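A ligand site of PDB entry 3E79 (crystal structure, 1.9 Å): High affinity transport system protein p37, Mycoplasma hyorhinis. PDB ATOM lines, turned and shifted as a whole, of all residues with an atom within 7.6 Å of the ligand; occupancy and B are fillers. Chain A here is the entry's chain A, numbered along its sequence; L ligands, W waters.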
ATOM      1  N   ASP A 164      14.519  -6.305 -15.907  1.00  0.00           N
ATOM      2  CA  ASP A 164      13.889  -5.211 -16.646  1.00  0.00           C
ATOM      3  C   ASP A 164      13.319  -5.655 -17.997  1.00  0.00           C
ATOM      4  O   ASP A 164      12.784  -4.827 -18.735  1.00  0.00           O
ATOM      5  CB  ASP A 164      14.879  -4.065 -16.856  1.00  0.00           C
ATOM      6  CG  ASP A 164      16.154  -4.516 -17.529  1.00  0.00           C
ATOM      7  OD1 ASP A 164      16.164  -5.564 -18.217  1.00  0.00           O
ATOM      8  OD2 ASP A 164      17.182  -3.812 -17.398  1.00  0.00           O
ATOM      9  N   GLY A 165      13.408  -6.923 -18.382  1.00  0.00           N
ATOM     10  CA  GLY A 165      12.809  -7.350 -19.639  1.00  0.00           C
ATOM     11  C   GLY A 165      13.633  -6.986 -20.851  1.00  0.00           C
ATOM     12  O   GLY A 165      13.158  -7.104 -21.988  1.00  0.00           O
ATOM     13  N   THR A 166      14.873  -6.555 -20.685  1.00  0.00           N
ATOM     14  CA  THR A 166      15.696  -6.256 -21.855  1.00  0.00           C
ATOM     15  C   THR A 166      16.540  -7.466 -22.224  1.00  0.00           C
ATOM     16  O   THR A 166      16.504  -8.522 -21.581  1.00  0.00           O
ATOM     17  CB  THR A 166      16.622  -5.046 -21.622  1.00  0.00           C
ATOM     18  OG1 THR A 166      17.574  -5.329 -20.574  1.00  0.00           O
ATOM     19  CG2 THR A 166      15.840  -3.834 -21.166  1.00  0.00           C
ATOM     20  N   ASP A 167      17.357  -7.337 -23.265  1.00  0.00           N
ATOM     21  CA  ASP A 167      18.123  -8.489 -23.746  1.00  0.00           C
ATOM     22  C   ASP A 167      19.121  -9.015 -22.738  1.00  0.00           C
ATOM     23  O   ASP A 167      19.632 -10.128 -22.913  1.00  0.00           O
ATOM     24  CB  ASP A 167      18.808  -8.124 -25.070  1.00  0.00           C
ATOM     25  CG  ASP A 167      20.226  -7.620 -24.905  1.00  0.00           C
ATOM     26  OD1 ASP A 167      21.173  -8.391 -25.154  1.00  0.00           O
ATOM     27  OD2 ASP A 167      20.403  -6.437 -24.520  1.00  0.00           O
ATOM     28  N   SER A 168      19.450  -8.293 -21.674  1.00  0.00           N
ATOM     29  CA  SER A 168      20.387  -8.821 -20.675  1.00  0.00           C
ATOM     30  C   SER A 168      19.654  -9.340 -19.446  1.00  0.00           C
ATOM     31  O   SER A 168      20.231  -9.713 -18.413  1.00  0.00           O
ATOM     32  CB  SER A 168      21.412  -7.755 -20.284  1.00  0.00           C
ATOM     33  OG  SER A 168      20.800  -6.598 -19.732  1.00  0.00           O
ATOM     34  N   ASP A 169      18.323  -9.364 -19.542  1.00  0.00           N
ATOM     35  CA  ASP A 169      17.515  -9.873 -18.423  1.00  0.00           C
ATOM     36  C   ASP A 169      17.684 -11.385 -18.367  1.00  0.00           C
ATOM     37  O   ASP A 169      17.626 -12.083 -19.384  1.00  0.00           O
ATOM     38  CB  ASP A 169      16.073  -9.439 -18.599  1.00  0.00           C
ATOM     39  CG  ASP A 169      15.170  -9.836 -17.453  1.00  0.00           C
ATOM     40  OD1 ASP A 169      15.073 -11.064 -17.246  1.00  0.00           O
ATOM     41  OD2 ASP A 169      14.576  -8.973 -16.780  1.00  0.00           O
ATOM     42  N   LEU A 171      15.816 -13.736 -17.432  1.00  0.00           N
ATOM     43  CA  LEU A 171      14.677 -14.515 -17.945  1.00  0.00           C
ATOM     44  C   LEU A 171      14.568 -14.421 -19.471  1.00  0.00           C
ATOM     45  O   LEU A 171      14.048 -15.331 -20.131  1.00  0.00           O
ATOM     46  CB  LEU A 171      13.350 -14.055 -17.333  1.00  0.00           C
ATOM     47  CG  LEU A 171      13.358 -14.005 -15.797  1.00  0.00           C
ATOM     48  CD1 LEU A 171      11.970 -13.727 -15.241  1.00  0.00           C
ATOM     49  CD2 LEU A 171      13.930 -15.310 -15.277  1.00  0.00           C
ATOM     50  N   VAL A 172      15.062 -13.317 -20.026  1.00  0.00           N
ATOM     51  CA  VAL A 172      15.089 -13.204 -21.492  1.00  0.00           C
ATOM     52  C   VAL A 172      16.162 -14.110 -22.060  1.00  0.00           C
ATOM     53  O   VAL A 172      15.946 -14.735 -23.102  1.00  0.00           O
ATOM     54  CB  VAL A 172      15.335 -11.762 -21.953  1.00  0.00           C
ATOM     55  CG1 VAL A 172      15.706 -11.741 -23.424  1.00  0.00           C
ATOM     56  CG2 VAL A 172      14.105 -10.893 -21.715  1.00  0.00           C
ATOM     57  N   LYS A 173      17.310 -14.177 -21.380  1.00  0.00           N
ATOM     58  CA  LYS A 173      18.387 -15.088 -21.768  1.00  0.00           C
ATOM     59  C   LYS A 173      17.949 -16.541 -21.771  1.00  0.00           C
ATOM     60  O   LYS A 173      18.271 -17.375 -22.632  1.00  0.00           O
ATOM     61  CB  LYS A 173      19.604 -14.931 -20.843  1.00  0.00           C
ATOM     62  CG  LYS A 173      20.153 -13.511 -20.787  1.00  0.00           C
ATOM     63  CD  LYS A 173      21.665 -13.471 -20.851  1.00  0.00           C
ATOM     64  CE  LYS A 173      22.174 -13.450 -22.288  1.00  0.00           C
ATOM     65  NZ  LYS A 173      22.484 -12.086 -22.786  1.00  0.00           N
ATOM     66  N   ALA A 175      14.860 -17.481 -22.317  1.00  0.00           N
ATOM     67  CA  ALA A 175      14.002 -17.588 -23.498  1.00  0.00           C
ATOM     68  C   ALA A 175      14.803 -17.728 -24.801  1.00  0.00           C
ATOM     69  O   ALA A 175      14.430 -18.455 -25.727  1.00  0.00           O
ATOM     70  CB  ALA A 175      13.082 -16.383 -23.562  1.00  0.00           C
ATOM     71  N   LYS A 176      15.933 -17.029 -24.899  1.00  0.00           N
ATOM     72  CA  LYS A 176      16.768 -17.179 -26.093  1.00  0.00           C
ATOM     73  C   LYS A 176      17.335 -18.588 -26.162  1.00  0.00           C
ATOM     74  O   LYS A 176      17.425 -19.168 -27.248  1.00  0.00           O
ATOM     75  CB  LYS A 176      17.850 -16.088 -26.093  1.00  0.00           C
ATOM     76  CG  LYS A 176      17.174 -14.727 -26.254  1.00  0.00           C
ATOM     77  CD  LYS A 176      18.099 -13.533 -26.151  1.00  0.00           C
ATOM     78  CE  LYS A 176      17.730 -12.495 -27.206  1.00  0.00           C
ATOM     79  NZ  LYS A 176      18.040 -11.121 -26.761  1.00  0.00           N
ATOM     80  N   ASN A 179      14.747 -20.803 -27.556  1.00  0.00           N
ATOM     81  CA  ASN A 179      14.551 -20.674 -29.008  1.00  0.00           C
ATOM     82  C   ASN A 179      15.626 -21.426 -29.797  1.00  0.00           C
ATOM     83  O   ASN A 179      15.356 -21.923 -30.890  1.00  0.00           O
ATOM     84  CB  ASN A 179      14.549 -19.192 -29.393  1.00  0.00           C
ATOM     85  CG  ASN A 179      13.302 -18.499 -28.891  1.00  0.00           C
ATOM     86  OD1 ASN A 179      12.297 -19.189 -28.704  1.00  0.00           O
ATOM     87  ND2 ASN A 179      13.357 -17.191 -28.686  1.00  0.00           N
ATOM     88  N   ILE A 219       6.169 -16.985 -21.764  1.00  0.00           N
ATOM     89  CA  ILE A 219       5.285 -16.308 -22.736  1.00  0.00           C
ATOM     90  C   ILE A 219       5.785 -16.591 -24.147  1.00  0.00           C
ATOM     91  O   ILE A 219       6.979 -16.389 -24.417  1.00  0.00           O
ATOM     92  CB  ILE A 219       5.207 -14.800 -22.452  1.00  0.00           C
ATOM     93  CG1 ILE A 219       4.603 -14.432 -21.092  1.00  0.00           C
ATOM     94  CG2 ILE A 219       4.433 -14.057 -23.545  1.00  0.00           C
ATOM     95  CD1 ILE A 219       4.756 -12.948 -20.785  1.00  0.00           C
ATOM     96  N   ILE A 221       5.298 -16.055 -28.433  1.00  0.00           N
ATOM     97  CA  ILE A 221       4.775 -15.060 -29.367  1.00  0.00           C
ATOM     98  C   ILE A 221       4.802 -15.690 -30.772  1.00  0.00           C
ATOM     99  O   ILE A 221       5.625 -16.569 -31.014  1.00  0.00           O
ATOM    100  CB  ILE A 221       5.520 -13.718 -29.434  1.00  0.00           C
ATOM    101  CG1 ILE A 221       6.995 -13.859 -29.830  1.00  0.00           C
ATOM    102  CG2 ILE A 221       5.361 -12.942 -28.132  1.00  0.00           C
ATOM    103  CD1 ILE A 221       7.789 -12.584 -29.710  1.00  0.00           C
ATOM    104  N   LEU A 228       6.198 -10.346 -35.581  1.00  0.00           N
ATOM    105  CA  LEU A 228       7.082 -10.593 -34.451  1.00  0.00           C
ATOM    106  C   LEU A 228       7.825  -9.324 -34.041  1.00  0.00           C
ATOM    107  O   LEU A 228       8.004  -8.973 -32.882  1.00  0.00           O
ATOM    108  CB  LEU A 228       8.075 -11.696 -34.832  1.00  0.00           C
ATOM    109  CG  LEU A 228       7.497 -13.108 -34.955  1.00  0.00           C
ATOM    110  CD1 LEU A 228       8.540 -14.072 -35.487  1.00  0.00           C
ATOM    111  CD2 LEU A 228       6.967 -13.605 -33.614  1.00  0.00           C
ATOM    112  N   ALA A 229       8.287  -8.573 -35.044  1.00  0.00           N
ATOM    113  CA  ALA A 229       9.077  -7.375 -34.710  1.00  0.00           C
ATOM    114  C   ALA A 229       8.197  -6.326 -34.033  1.00  0.00           C
ATOM    115  O   ALA A 229       8.624  -5.631 -33.126  1.00  0.00           O
ATOM    116  CB  ALA A 229       9.728  -6.810 -35.959  1.00  0.00           C
ATOM    117  N   LYS A 232       7.755  -7.325 -30.468  1.00  0.00           N
ATOM    118  CA  LYS A 232       8.923  -7.016 -29.613  1.00  0.00           C
ATOM    119  C   LYS A 232       9.087  -5.516 -29.420  1.00  0.00           C
ATOM    120  O   LYS A 232       9.455  -5.030 -28.354  1.00  0.00           O
ATOM    121  CB  LYS A 232      10.174  -7.669 -30.214  1.00  0.00           C
ATOM    122  CG  LYS A 232      10.030  -9.183 -30.240  1.00  0.00           C
ATOM    123  CD  LYS A 232      11.366  -9.883 -30.341  1.00  0.00           C
ATOM    124  CE  LYS A 232      11.713 -10.276 -31.756  1.00  0.00           C
ATOM    125  NZ  LYS A 232      12.115 -11.701 -31.867  1.00  0.00           N
ATOM    126  N   LYS A 233       8.773  -4.751 -30.482  1.00  0.00           N
ATOM    127  CA  LYS A 233       8.758  -3.307 -30.316  1.00  0.00           C
ATOM    128  C   LYS A 233       7.767  -2.843 -29.249  1.00  0.00           C
ATOM    129  O   LYS A 233       8.084  -1.997 -28.421  1.00  0.00           O
ATOM    130  CB  LYS A 233       8.363  -2.561 -31.602  1.00  0.00           C
ATOM    131  CG  LYS A 233       7.856  -1.165 -31.250  1.00  0.00           C
ATOM    132  CD  LYS A 233       6.528  -0.818 -31.883  1.00  0.00           C
ATOM    133  CE  LYS A 233       5.319  -1.473 -31.245  1.00  0.00           C
ATOM    134  NZ  LYS A 233       4.461  -2.140 -32.265  1.00  0.00           N
ATOM    135  N   TRP A 235       6.717  -4.453 -26.719  1.00  0.00           N
ATOM    136  CA  TRP A 235       7.328  -4.907 -25.487  1.00  0.00           C
ATOM    137  C   TRP A 235       8.460  -3.971 -25.067  1.00  0.00           C
ATOM    138  O   TRP A 235       8.550  -3.516 -23.924  1.00  0.00           O
ATOM    139  CB  TRP A 235       7.893  -6.327 -25.656  1.00  0.00           C
ATOM    140  CG  TRP A 235       8.652  -6.829 -24.464  1.00  0.00           C
ATOM    141  CD1 TRP A 235      10.004  -6.765 -24.265  1.00  0.00           C
ATOM    142  CD2 TRP A 235       8.115  -7.479 -23.293  1.00  0.00           C
ATOM    143  NE1 TRP A 235      10.327  -7.330 -23.048  1.00  0.00           N
ATOM    144  CE2 TRP A 235       9.187  -7.773 -22.434  1.00  0.00           C
ATOM    145  CE3 TRP A 235       6.819  -7.832 -22.899  1.00  0.00           C
ATOM    146  CZ2 TRP A 235       9.028  -8.407 -21.187  1.00  0.00           C
ATOM    147  CZ3 TRP A 235       6.668  -8.463 -21.672  1.00  0.00           C
ATOM    148  CH2 TRP A 235       7.762  -8.741 -20.846  1.00  0.00           C
ATOM    149  N   ASN A 236       9.339  -3.677 -26.027  1.00  0.00           N
ATOM    150  CA  ASN A 236      10.427  -2.753 -25.630  1.00  0.00           C
ATOM    151  C   ASN A 236       9.940  -1.336 -25.359  1.00  0.00           C
ATOM    152  O   ASN A 236      10.503  -0.669 -24.492  1.00  0.00           O
ATOM    153  CB  ASN A 236      11.510  -2.768 -26.715  1.00  0.00           C
ATOM    154  CG  ASN A 236      12.243  -4.095 -26.730  1.00  0.00           C
ATOM    155  OD1 ASN A 236      12.602  -4.633 -25.689  1.00  0.00           O
ATOM    156  ND2 ASN A 236      12.448  -4.615 -27.926  1.00  0.00           N
ATOM    157  N   HIS A 269       6.651  -5.396 -16.086  1.00  0.00           N
ATOM    158  CA  HIS A 269       7.282  -4.844 -17.286  1.00  0.00           C
ATOM    159  C   HIS A 269       6.513  -3.610 -17.758  1.00  0.00           C
ATOM    160  O   HIS A 269       7.124  -2.589 -18.049  1.00  0.00           O
ATOM    161  CB  HIS A 269       7.368  -5.869 -18.411  1.00  0.00           C
ATOM    162  CG  HIS A 269       8.134  -5.335 -19.592  1.00  0.00           C
ATOM    163  ND1 HIS A 269       9.501  -5.185 -19.557  1.00  0.00           N
ATOM    164  CD2 HIS A 269       7.749  -4.908 -20.817  1.00  0.00           C
ATOM    165  CE1 HIS A 269       9.930  -4.699 -20.720  1.00  0.00           C
ATOM    166  NE2 HIS A 269       8.880  -4.521 -21.503  1.00  0.00           N
ATOM    167  N   GLU A 333       7.805 -18.447 -30.978  1.00  0.00           N
ATOM    168  CA  GLU A 333       9.062 -18.458 -30.231  1.00  0.00           C
ATOM    169  C   GLU A 333       8.826 -17.909 -28.828  1.00  0.00           C
ATOM    170  O   GLU A 333       7.776 -17.279 -28.644  1.00  0.00           O
ATOM    171  CB  GLU A 333      10.146 -17.677 -30.959  1.00  0.00           C
ATOM    172  CG  GLU A 333       9.983 -16.179 -30.971  1.00  0.00           C
ATOM    173  CD  GLU A 333      10.744 -15.489 -32.088  1.00  0.00           C
ATOM    174  OE1 GLU A 333      10.858 -14.248 -32.018  1.00  0.00           O
ATOM    175  OE2 GLU A 333      11.232 -16.111 -33.056  1.00  0.00           O
ATOM    176  N   ALA A 334       9.793 -18.172 -27.956  1.00  0.00           N
ATOM    177  CA  ALA A 334       9.701 -17.712 -26.572  1.00  0.00           C
ATOM    178  C   ALA A 334      10.102 -16.256 -26.475  1.00  0.00           C
ATOM    179  O   ALA A 334      11.098 -15.833 -27.075  1.00  0.00           O
ATOM    180  CB  ALA A 334      10.554 -18.577 -25.649  1.00  0.00           C
ATOM    181  N   LEU A 335       9.325 -15.491 -25.705  1.00  0.00           N
ATOM    182  CA  LEU A 335       9.667 -14.092 -25.476  1.00  0.00           C
ATOM    183  C   LEU A 335      10.427 -13.941 -24.166  1.00  0.00           C
ATOM    184  O   LEU A 335      11.465 -13.286 -24.107  1.00  0.00           O
ATOM    185  CB  LEU A 335       8.405 -13.237 -25.481  1.00  0.00           C
ATOM    186  CG  LEU A 335       8.576 -11.763 -25.111  1.00  0.00           C
ATOM    187  CD1 LEU A 335       9.201 -11.012 -26.278  1.00  0.00           C
ATOM    188  CD2 LEU A 335       7.238 -11.155 -24.716  1.00  0.00           C
ATOM    189  N   ILE A 336       9.880 -14.540 -23.116  1.00  0.00           N
ATOM    190  CA  ILE A 336      10.489 -14.474 -21.791  1.00  0.00           C
ATOM    191  C   ILE A 336       9.900 -15.560 -20.891  1.00  0.00           C
ATOM    192  O   ILE A 336       8.786 -16.033 -21.175  1.00  0.00           O
ATOM    193  CB  ILE A 336      10.259 -13.089 -21.183  1.00  0.00           C
ATOM    194  CG1 ILE A 336      10.993 -12.807 -19.859  1.00  0.00           C
ATOM    195  CG2 ILE A 336       8.761 -12.848 -20.992  1.00  0.00           C
ATOM    196  CD1 ILE A 336      10.970 -11.343 -19.459  1.00  0.00           C
HETATM  197  I1  LIG L   1      13.757  -8.077 -25.460  1.00  0.00           I
HETATM  198  I2  LIG L   1      13.132 -13.622 -27.591  1.00  0.00           I
HETATM  199  I3  LIG L   1      16.301  -9.607 -30.721  1.00  0.00           I
HETATM  200  O1  LIG L   1      16.293  -7.256 -27.587  1.00  0.00           O
HETATM  201  O2  LIG L   1      14.504  -6.984 -28.916  1.00  0.00           O
HETATM  202  C1  LIG L   1      14.995 -12.483 -29.928  1.00  0.00           C
HETATM  203  N1  LIG L   1      12.878 -11.080 -25.685  1.00  0.00           N
HETATM  204  C2  LIG L   1      14.896  -9.141 -28.051  1.00  0.00           C
HETATM  205  C3  LIG L   1      14.177  -9.510 -26.911  1.00  0.00           C
HETATM  206  C4  LIG L   1      13.665 -10.796 -26.735  1.00  0.00           C
HETATM  207  C5  LIG L   1      13.997 -11.736 -27.711  1.00  0.00           C
HETATM  208  C6  LIG L   1      14.687 -11.394 -28.881  1.00  0.00           C
HETATM  209  C7  LIG L   1      15.177 -10.096 -29.031  1.00  0.00           C
HETATM  210  C8  LIG L   1      15.281  -7.649 -28.192  1.00  0.00           C
HETATM  211  O3  LIG L   1      14.270 -12.558 -30.935  1.00  0.00           O
HETATM  212  O4  LIG L   1      15.971 -13.211 -29.691  1.00  0.00           O
HETATM  213  O   HOH W   1      15.776 -16.159 -29.666  1.00  0.00           O
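O of Lys 232 is in hydrogen-bond range of ND2 of Asn 236, 3.1 Å away. NZ of Lys 232 is in salt-bridge range of OE1 of Glu 333, at 2.8 Å. The backbone NH (N) of Ala 334 is in hydrogen-bond range of the side-chain amide oxygen (OD1) of Asn 179 (2.8 Å). The backbone carbonyl oxygen (O) of Ile 219 sits at hydrogen-bond distance from the backbone NH (N) of Leu 335. The indole nitrogen of Trp 235 lies within hydrogen-bond range of the backbone carbonyl oxygen of Gly 165 (3.0 Å). The backbone NH of Gly 165 is in hydrogen-bond range of the side-chain carboxylate of Asp 169. The side-chain amino group of Lys 173 is in hydrogen-bond range of the backbone carbonyl oxygen of Asp 167 (3.5 Å). The backbone carbonyl oxygen (O) of Glu 333 lies within hydrogen-bond range of the backbone NH (N) of Ile 221 (2.8 Å).
Residues that only touch the ligand: Ala 334, Lys 176, Gly 165, Asp 167, Val 172, Asn 179 and Glu 333. Within 4 Å of the ligand: Gly 165, Asp 167, Val 172, Lys 176, Asn 179, Lys 232, Asn 236, Glu 333, Ala 334 and Leu 335. The nearest printed residue that does not touch the ligand is Trp 235 (4.2 Å).
The side-chain amino group (NZ) of Lys 232 is in salt-bridge range of an oxygen (O3) of the ligand, at 2.5 Å. The backbone carbonyl oxygen (O) of Leu 335 sits at hydrogen-bond distance from a nitrogen (N1) of the ligand, at 3.1 Å. The side-chain amide nitrogen (ND2) of Asn 236 is in hydrogen-bond range of an oxygen (O2) of the ligand.
Water W1 bridges the side-chain amide nitrogen (ND2) of Asn 179 (2.8 Å) and an oxygen (O4) of the ligand (3.0 Å).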
